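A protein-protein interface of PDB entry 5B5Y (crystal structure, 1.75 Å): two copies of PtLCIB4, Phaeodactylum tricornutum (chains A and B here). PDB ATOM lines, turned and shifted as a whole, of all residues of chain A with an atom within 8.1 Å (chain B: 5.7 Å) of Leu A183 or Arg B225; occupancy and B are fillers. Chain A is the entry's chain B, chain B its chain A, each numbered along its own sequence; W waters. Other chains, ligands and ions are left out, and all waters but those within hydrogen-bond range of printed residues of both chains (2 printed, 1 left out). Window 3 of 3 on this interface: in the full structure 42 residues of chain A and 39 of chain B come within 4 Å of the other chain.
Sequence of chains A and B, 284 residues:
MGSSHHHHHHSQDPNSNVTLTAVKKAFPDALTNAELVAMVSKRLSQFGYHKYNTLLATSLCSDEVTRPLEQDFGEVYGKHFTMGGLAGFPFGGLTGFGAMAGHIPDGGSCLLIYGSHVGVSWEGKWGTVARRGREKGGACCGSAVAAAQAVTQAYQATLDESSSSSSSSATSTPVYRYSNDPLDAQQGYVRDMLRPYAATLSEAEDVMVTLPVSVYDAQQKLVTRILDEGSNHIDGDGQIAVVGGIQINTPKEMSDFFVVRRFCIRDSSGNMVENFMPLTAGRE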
ATOM      1  N   LEU A  86      13.993 -12.639 -12.744  1.00  0.00           N
ATOM      2  CA  LEU A  86      14.274 -11.955 -11.478  1.00  0.00           C
ATOM      3  C   LEU A  86      14.730 -12.903 -10.367  1.00  0.00           C
ATOM      4  O   LEU A  86      14.113 -13.944 -10.140  1.00  0.00           O
ATOM      5  CB  LEU A  86      13.034 -11.193 -11.011  1.00  0.00           C
ATOM      6  CG  LEU A  86      12.556 -10.095 -11.958  1.00  0.00           C
ATOM      7  CD1 LEU A  86      11.411  -9.350 -11.288  1.00  0.00           C
ATOM      8  CD2 LEU A  86      13.670  -9.128 -12.317  1.00  0.00           C
ATOM      9  N   ASP A 181      -1.607 -10.681 -14.967  1.00  0.00           N
ATOM     10  CA  ASP A 181      -1.048  -9.521 -15.667  1.00  0.00           C
ATOM     11  C   ASP A 181       0.480  -9.566 -15.640  1.00  0.00           C
ATOM     12  O   ASP A 181       1.099  -9.470 -14.575  1.00  0.00           O
ATOM     13  CB  ASP A 181      -1.568  -8.220 -15.048  1.00  0.00           C
ATOM     14  CG  ASP A 181      -1.073  -6.970 -15.775  1.00  0.00           C
ATOM     15  OD1 ASP A 181      -0.483  -7.078 -16.871  1.00  0.00           O
ATOM     16  OD2 ASP A 181      -1.288  -5.861 -15.239  1.00  0.00           O
ATOM     17  N   PRO A 182       1.095  -9.709 -16.823  1.00  0.00           N
ATOM     18  CA  PRO A 182       2.549  -9.905 -16.882  1.00  0.00           C
ATOM     19  C   PRO A 182       3.354  -8.640 -16.587  1.00  0.00           C
ATOM     20  O   PRO A 182       4.571  -8.739 -16.443  1.00  0.00           O
ATOM     21  CB  PRO A 182       2.778 -10.365 -18.323  1.00  0.00           C
ATOM     22  CG  PRO A 182       1.687  -9.677 -19.098  1.00  0.00           C
ATOM     23  CD  PRO A 182       0.481  -9.692 -18.164  1.00  0.00           C
ATOM     24  N   LEU A 183       2.697  -7.487 -16.496  1.00  0.00           N
ATOM     25  CA  LEU A 183       3.409  -6.226 -16.258  1.00  0.00           C
ATOM     26  C   LEU A 183       4.384  -6.298 -15.085  1.00  0.00           C
ATOM     27  O   LEU A 183       5.478  -5.743 -15.156  1.00  0.00           O
ATOM     28  CB  LEU A 183       2.430  -5.093 -16.007  1.00  0.00           C
ATOM     29  CG  LEU A 183       3.119  -3.741 -16.099  1.00  0.00           C
ATOM     30  CD1 LEU A 183       3.724  -3.563 -17.502  1.00  0.00           C
ATOM     31  CD2 LEU A 183       2.134  -2.629 -15.795  1.00  0.00           C
ATOM     32  N   ASP A 184       3.988  -6.963 -14.005  1.00  0.00           N
ATOM     33  CA  ASP A 184       4.914  -7.171 -12.885  1.00  0.00           C
ATOM     34  C   ASP A 184       4.751  -8.545 -12.236  1.00  0.00           C
ATOM     35  O   ASP A 184       4.986  -8.714 -11.032  1.00  0.00           O
ATOM     36  CB  ASP A 184       4.739  -6.074 -11.830  1.00  0.00           C
ATOM     37  CG  ASP A 184       6.039  -5.733 -11.120  1.00  0.00           C
ATOM     38  OD1 ASP A 184       7.115  -6.042 -11.665  1.00  0.00           O
ATOM     39  OD2 ASP A 184       5.988  -5.147 -10.018  1.00  0.00           O
ATOM     40  N   ALA A 185       4.369  -9.530 -13.040  1.00  0.00           N
ATOM     41  CA  ALA A 185       4.044 -10.850 -12.514  1.00  0.00           C
ATOM     42  C   ALA A 185       5.252 -11.562 -11.900  1.00  0.00           C
ATOM     43  O   ALA A 185       5.128 -12.200 -10.851  1.00  0.00           O
ATOM     44  CB  ALA A 185       3.417 -11.710 -13.612  1.00  0.00           C
ATOM     45  N   GLN A 186       6.421 -11.456 -12.535  1.00  0.00           N
ATOM     46  CA  GLN A 186       7.604 -12.146 -12.026  1.00  0.00           C
ATOM     47  C   GLN A 186       7.965 -11.774 -10.604  1.00  0.00           C
ATOM     48  O   GLN A 186       8.211 -12.656  -9.790  1.00  0.00           O
ATOM     49  CB  GLN A 186       8.822 -11.904 -12.934  1.00  0.00           C
ATOM     50  CG  GLN A 186       9.191 -13.146 -13.698  1.00  0.00           C
ATOM     51  CD  GLN A 186      10.417 -13.022 -14.578  1.00  0.00           C
ATOM     52  OE1 GLN A 186      11.395 -12.343 -14.255  1.00  0.00           O
ATOM     53  NE2 GLN A 186      10.348 -13.670 -15.731  1.00  0.00           N
ATOM     54  N   GLN A 187       8.006 -10.475 -10.293  1.00  0.00           N
ATOM     55  CA  GLN A 187       8.344 -10.052  -8.945  1.00  0.00           C
ATOM     56  C   GLN A 187       7.287 -10.543  -7.957  1.00  0.00           C
ATOM     57  O   GLN A 187       7.599 -10.812  -6.796  1.00  0.00           O
ATOM     58  CB  GLN A 187       8.489  -8.530  -8.852  1.00  0.00           C
ATOM     59  CG  GLN A 187       8.954  -8.024  -7.479  1.00  0.00           C
ATOM     60  CD  GLN A 187      10.322  -8.569  -7.071  1.00  0.00           C
ATOM     61  OE1 GLN A 187      11.044  -9.141  -7.884  1.00  0.00           O
ATOM     62  NE2 GLN A 187      10.687  -8.373  -5.805  1.00  0.00           N
ATOM     63  N   GLY B  92      10.620  -9.513 -17.359  1.00  0.00           N
ATOM     64  CA  GLY B  92      11.198  -8.878 -16.185  1.00  0.00           C
ATOM     65  C   GLY B  92      10.248  -7.807 -15.657  1.00  0.00           C
ATOM     66  O   GLY B  92      10.244  -7.497 -14.459  1.00  0.00           O
ATOM     67  N   GLY B  93       9.437  -7.252 -16.558  1.00  0.00           N
ATOM     68  CA  GLY B  93       8.390  -6.311 -16.185  1.00  0.00           C
ATOM     69  C   GLY B  93       8.849  -5.025 -15.518  1.00  0.00           C
ATOM     70  O   GLY B  93       9.978  -4.578 -15.696  1.00  0.00           O
ATOM     71  N   LEU B  94       7.948  -4.424 -14.746  1.00  0.00           N
ATOM     72  CA  LEU B  94       8.211  -3.135 -14.109  1.00  0.00           C
ATOM     73  C   LEU B  94       9.349  -3.199 -13.112  1.00  0.00           C
ATOM     74  O   LEU B  94      10.188  -2.300 -13.057  1.00  0.00           O
ATOM     75  CB  LEU B  94       6.956  -2.629 -13.399  1.00  0.00           C
ATOM     76  CG  LEU B  94       5.944  -1.928 -14.289  1.00  0.00           C
ATOM     77  CD1 LEU B  94       4.825  -1.340 -13.428  1.00  0.00           C
ATOM     78  CD2 LEU B  94       6.674  -0.854 -15.076  1.00  0.00           C
ATOM     79  N   THR B  95       9.367  -4.249 -12.301  1.00  0.00           N
ATOM     80  CA  THR B  95      10.433  -4.401 -11.307  1.00  0.00           C
ATOM     81  C   THR B  95      11.781  -4.575 -11.993  1.00  0.00           C
ATOM     82  O   THR B  95      12.761  -3.941 -11.607  1.00  0.00           O
ATOM     83  CB  THR B  95      10.168  -5.583 -10.354  1.00  0.00           C
ATOM     84  OG1 THR B  95       9.033  -5.279  -9.521  1.00  0.00           O
ATOM     85  CG2 THR B  95      11.368  -5.829  -9.452  1.00  0.00           C
ATOM     86  N   GLN B 220       5.814  -4.895 -28.586  1.00  0.00           N
ATOM     87  CA  GLN B 220       6.040  -3.449 -28.601  1.00  0.00           C
ATOM     88  C   GLN B 220       5.009  -2.748 -27.725  1.00  0.00           C
ATOM     89  O   GLN B 220       5.322  -1.759 -27.072  1.00  0.00           O
ATOM     90  CB  GLN B 220       6.040  -2.889 -30.027  1.00  0.00           C
ATOM     91  CG  GLN B 220       4.726  -2.953 -30.768  1.00  0.00           C
ATOM     92  CD  GLN B 220       3.880  -1.708 -30.563  1.00  0.00           C
ATOM     93  OE1 GLN B 220       4.370  -0.686 -30.083  1.00  0.00           O
ATOM     94  NE2 GLN B 220       2.603  -1.795 -30.916  1.00  0.00           N
ATOM     95  N   LYS B 221       3.796  -3.297 -27.677  1.00  0.00           N
ATOM     96  CA  LYS B 221       2.776  -2.790 -26.756  1.00  0.00           C
ATOM     97  C   LYS B 221       3.166  -2.955 -25.286  1.00  0.00           C
ATOM     98  O   LYS B 221       2.988  -2.026 -24.493  1.00  0.00           O
ATOM     99  CB  LYS B 221       1.437  -3.478 -27.024  1.00  0.00           C
ATOM    100  CG  LYS B 221       0.855  -3.059 -28.353  1.00  0.00           C
ATOM    101  CD  LYS B 221      -0.473  -3.737 -28.636  1.00  0.00           C
ATOM    102  CE  LYS B 221      -1.007  -3.323 -30.002  1.00  0.00           C
ATOM    103  NZ  LYS B 221      -2.023  -4.292 -30.513  1.00  0.00           N
ATOM    104  N   LEU B 222       3.694  -4.120 -24.918  1.00  0.00           N
ATOM    105  CA  LEU B 222       4.118  -4.340 -23.533  1.00  0.00           C
ATOM    106  C   LEU B 222       5.339  -3.487 -23.185  1.00  0.00           C
ATOM    107  O   LEU B 222       5.409  -2.926 -22.103  1.00  0.00           O
ATOM    108  CB  LEU B 222       4.423  -5.821 -23.286  1.00  0.00           C
ATOM    109  CG  LEU B 222       4.830  -6.250 -21.876  1.00  0.00           C
ATOM    110  CD1 LEU B 222       3.807  -5.786 -20.843  1.00  0.00           C
ATOM    111  CD2 LEU B 222       4.979  -7.772 -21.819  1.00  0.00           C
ATOM    112  N   VAL B 223       6.294  -3.382 -24.104  1.00  0.00           N
ATOM    113  CA  VAL B 223       7.468  -2.541 -23.865  1.00  0.00           C
ATOM    114  C   VAL B 223       7.057  -1.084 -23.617  1.00  0.00           C
ATOM    115  O   VAL B 223       7.500  -0.448 -22.648  1.00  0.00           O
ATOM    116  CB  VAL B 223       8.459  -2.622 -25.051  1.00  0.00           C
ATOM    117  CG1 VAL B 223       9.529  -1.550 -24.933  1.00  0.00           C
ATOM    118  CG2 VAL B 223       9.087  -3.996 -25.083  1.00  0.00           C
ATOM    119  N   THR B 224       6.171  -0.574 -24.455  1.00  0.00           N
ATOM    120  CA  THR B 224       5.692   0.793 -24.298  1.00  0.00           C
ATOM    121  C   THR B 224       5.026   0.976 -22.932  1.00  0.00           C
ATOM    122  O   THR B 224       5.304   1.944 -22.232  1.00  0.00           O
ATOM    123  CB  THR B 224       4.724   1.173 -25.431  1.00  0.00           C
ATOM    124  OG1 THR B 224       5.432   1.103 -26.677  1.00  0.00           O
ATOM    125  CG2 THR B 224       4.194   2.601 -25.247  1.00  0.00           C
ATOM    126  N   ARG B 225       4.179   0.028 -22.538  1.00  0.00           N
ATOM    127  CA  ARG B 225       3.565   0.094 -21.211  1.00  0.00           C
ATOM    128  C   ARG B 225       4.585   0.114 -20.078  1.00  0.00           C
ATOM    129  O   ARG B 225       4.457   0.901 -19.140  1.00  0.00           O
ATOM    130  CB  ARG B 225       2.592  -1.077 -21.009  1.00  0.00           C
ATOM    131  CG  ARG B 225       1.882  -1.078 -19.647  1.00  0.00           C
ATOM    132  CD  ARG B 225       0.703  -2.065 -19.655  1.00  0.00           C
ATOM    133  NE  ARG B 225      -0.386  -1.583 -20.502  1.00  0.00           N
ATOM    134  CZ  ARG B 225      -1.446  -2.301 -20.867  1.00  0.00           C
ATOM    135  NH1 ARG B 225      -1.575  -3.567 -20.477  1.00  0.00           N
ATOM    136  NH2 ARG B 225      -2.385  -1.748 -21.627  1.00  0.00           N
ATOM    137  N   ILE B 226       5.598  -0.750 -20.154  1.00  0.00           N
ATOM    138  CA  ILE B 226       6.637  -0.777 -19.129  1.00  0.00           C
ATOM    139  C   ILE B 226       7.391   0.562 -19.067  1.00  0.00           C
ATOM    140  O   ILE B 226       7.623   1.113 -17.984  1.00  0.00           O
ATOM    141  CB  ILE B 226       7.630  -1.929 -19.385  1.00  0.00           C
ATOM    142  CG1 ILE B 226       6.949  -3.273 -19.102  1.00  0.00           C
ATOM    143  CG2 ILE B 226       8.854  -1.780 -18.507  1.00  0.00           C
ATOM    144  CD1 ILE B 226       7.710  -4.454 -19.688  1.00  0.00           C
ATOM    145  N   LEU B 227       7.746   1.092 -20.233  1.00  0.00           N
ATOM    146  CA  LEU B 227       8.471   2.357 -20.284  1.00  0.00           C
ATOM    147  C   LEU B 227       7.619   3.521 -19.762  1.00  0.00           C
ATOM    148  O   LEU B 227       8.142   4.412 -19.101  1.00  0.00           O
ATOM    149  CB  LEU B 227       8.936   2.666 -21.704  1.00  0.00           C
ATOM    150  CG  LEU B 227       9.909   1.676 -22.340  1.00  0.00           C
ATOM    151  CD1 LEU B 227      10.183   2.080 -23.781  1.00  0.00           C
ATOM    152  CD2 LEU B 227      11.199   1.617 -21.548  1.00  0.00           C
ATOM    153  N   ASP B 228       6.324   3.511 -20.073  1.00  0.00           N
ATOM    154  CA  ASP B 228       5.394   4.508 -19.539  1.00  0.00           C
ATOM    155  C   ASP B 228       5.286   4.424 -18.019  1.00  0.00           C
ATOM    156  O   ASP B 228       5.382   5.439 -17.323  1.00  0.00           O
ATOM    157  CB  ASP B 228       4.000   4.345 -20.164  1.00  0.00           C
ATOM    158  CG  ASP B 228       3.954   4.788 -21.612  1.00  0.00           C
ATOM    159  OD1 ASP B 228       4.954   5.362 -22.095  1.00  0.00           O
ATOM    160  OD2 ASP B 228       2.918   4.561 -22.274  1.00  0.00           O
ATOM    161  N   GLU B 229       5.097   3.214 -17.499  1.00  0.00           N
ATOM    162  CA  GLU B 229       4.899   3.021 -16.060  1.00  0.00           C
ATOM    163  C   GLU B 229       6.177   3.248 -15.259  1.00  0.00           C
ATOM    164  O   GLU B 229       6.118   3.610 -14.087  1.00  0.00           O
ATOM    165  CB  GLU B 229       4.377   1.612 -15.772  1.00  0.00           C
ATOM    166  CG  GLU B 229       3.015   1.296 -16.355  1.00  0.00           C
ATOM    167  CD  GLU B 229       1.880   1.702 -15.437  1.00  0.00           C
ATOM    168  OE1 GLU B 229       2.141   1.951 -14.237  1.00  0.00           O
ATOM    169  OE2 GLU B 229       0.736   1.759 -15.921  1.00  0.00           O
ATOM    170  N   GLY B 230       7.330   3.032 -15.891  1.00  0.00           N
ATOM    171  CA  GLY B 230       8.597   3.049 -15.175  1.00  0.00           C
ATOM    172  C   GLY B 230       9.412   4.302 -15.435  1.00  0.00           C
ATOM    173  O   GLY B 230      10.579   4.380 -15.050  1.00  0.00           O
HETATM  174  O   HOH W   1       0.227  -5.515 -19.187  1.00  0.00           O
HETATM  175  O   HOH W   2       7.992  -8.462 -12.650  1.00  0.00           O
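N of Leu A86 sits at hydrogen-bond distance from OE1 of Gln A186 (3.0 Å).
The side-chain carboxylate (OD1) of Asp A181 lies close to the backbone NH (N) of Leu A183, 3.2 Å away.
No position is printed for both chains.
O of Leu A183 lies within hydrogen-bond range of N of Leu B94 (2.8 Å).
The backbone NH (N) of Thr B95 sits at hydrogen-bond distance from the side-chain carboxylate (OD1) of Asp A184 (2.9 Å).
Of chain A, only Leu A183 comes within 4 Å of Arg B225.
Of the printed residues of chain B, Leu A86 touches Gly B92 (3.9 Å) and Thr B95 (3.97 Å).
Of the printed residues of chain B, Asp A184 touches Leu B94 (3.6 Å) and Thr B95 (2.9 Å).
Of the printed residues of chain B, Gln A187 touches Thr B95 (3.4 Å).
Gln B220 touches none of the printed residues of chain A.
Asp A181 touches none of the printed residues of chain B.
The nearest printed residue of chain B that does not touch Leu A183 is Leu B222 (4.01 Å).
The nearest printed residue of chain A that does not touch Gly B93 is Asp A184 (4.3 Å).
Water W2 lies within hydrogen-bond range of OD1 of Asp A184 (2.8 Å), O of Gly B92 (3.0 Å), N of Gln A187 (3.1 Å) and N of Gln A186 (3.4 Å).
Water W1 bridges the side-chain carboxylate of Asp A181 and the guanidinium group of Arg B225.
Among the printed residues, merely in contact across the chains: Leu A86 with Gly B92 (3.9 Å), Leu A86 with Thr B95 (3.97 Å), Leu A183 with Gly B93 (3.1 Å), Leu A183 with Arg B225 (3.8 Å), Leu A183 with Ile B226 (3.6 Å), Asp A184 with Leu B94 (3.6 Å), Gln A186 with Gly B92 (3.97 Å) and Gln A187 with Thr B95 (3.4 Å).
Of the 15 printed residues of chain B, 6 touch a printed residue of chain A.
Printed residues of chain A that touch a printed residue of chain B: Leu A86, Leu A183, Asp A184, Gln A186 and Gln A187.
Hydrophobic or aromatic side chains of chain A that line the printed part of chain B: Leu A86 and Leu A183.
Among the printed residues, 10 pairs touch across the chains.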
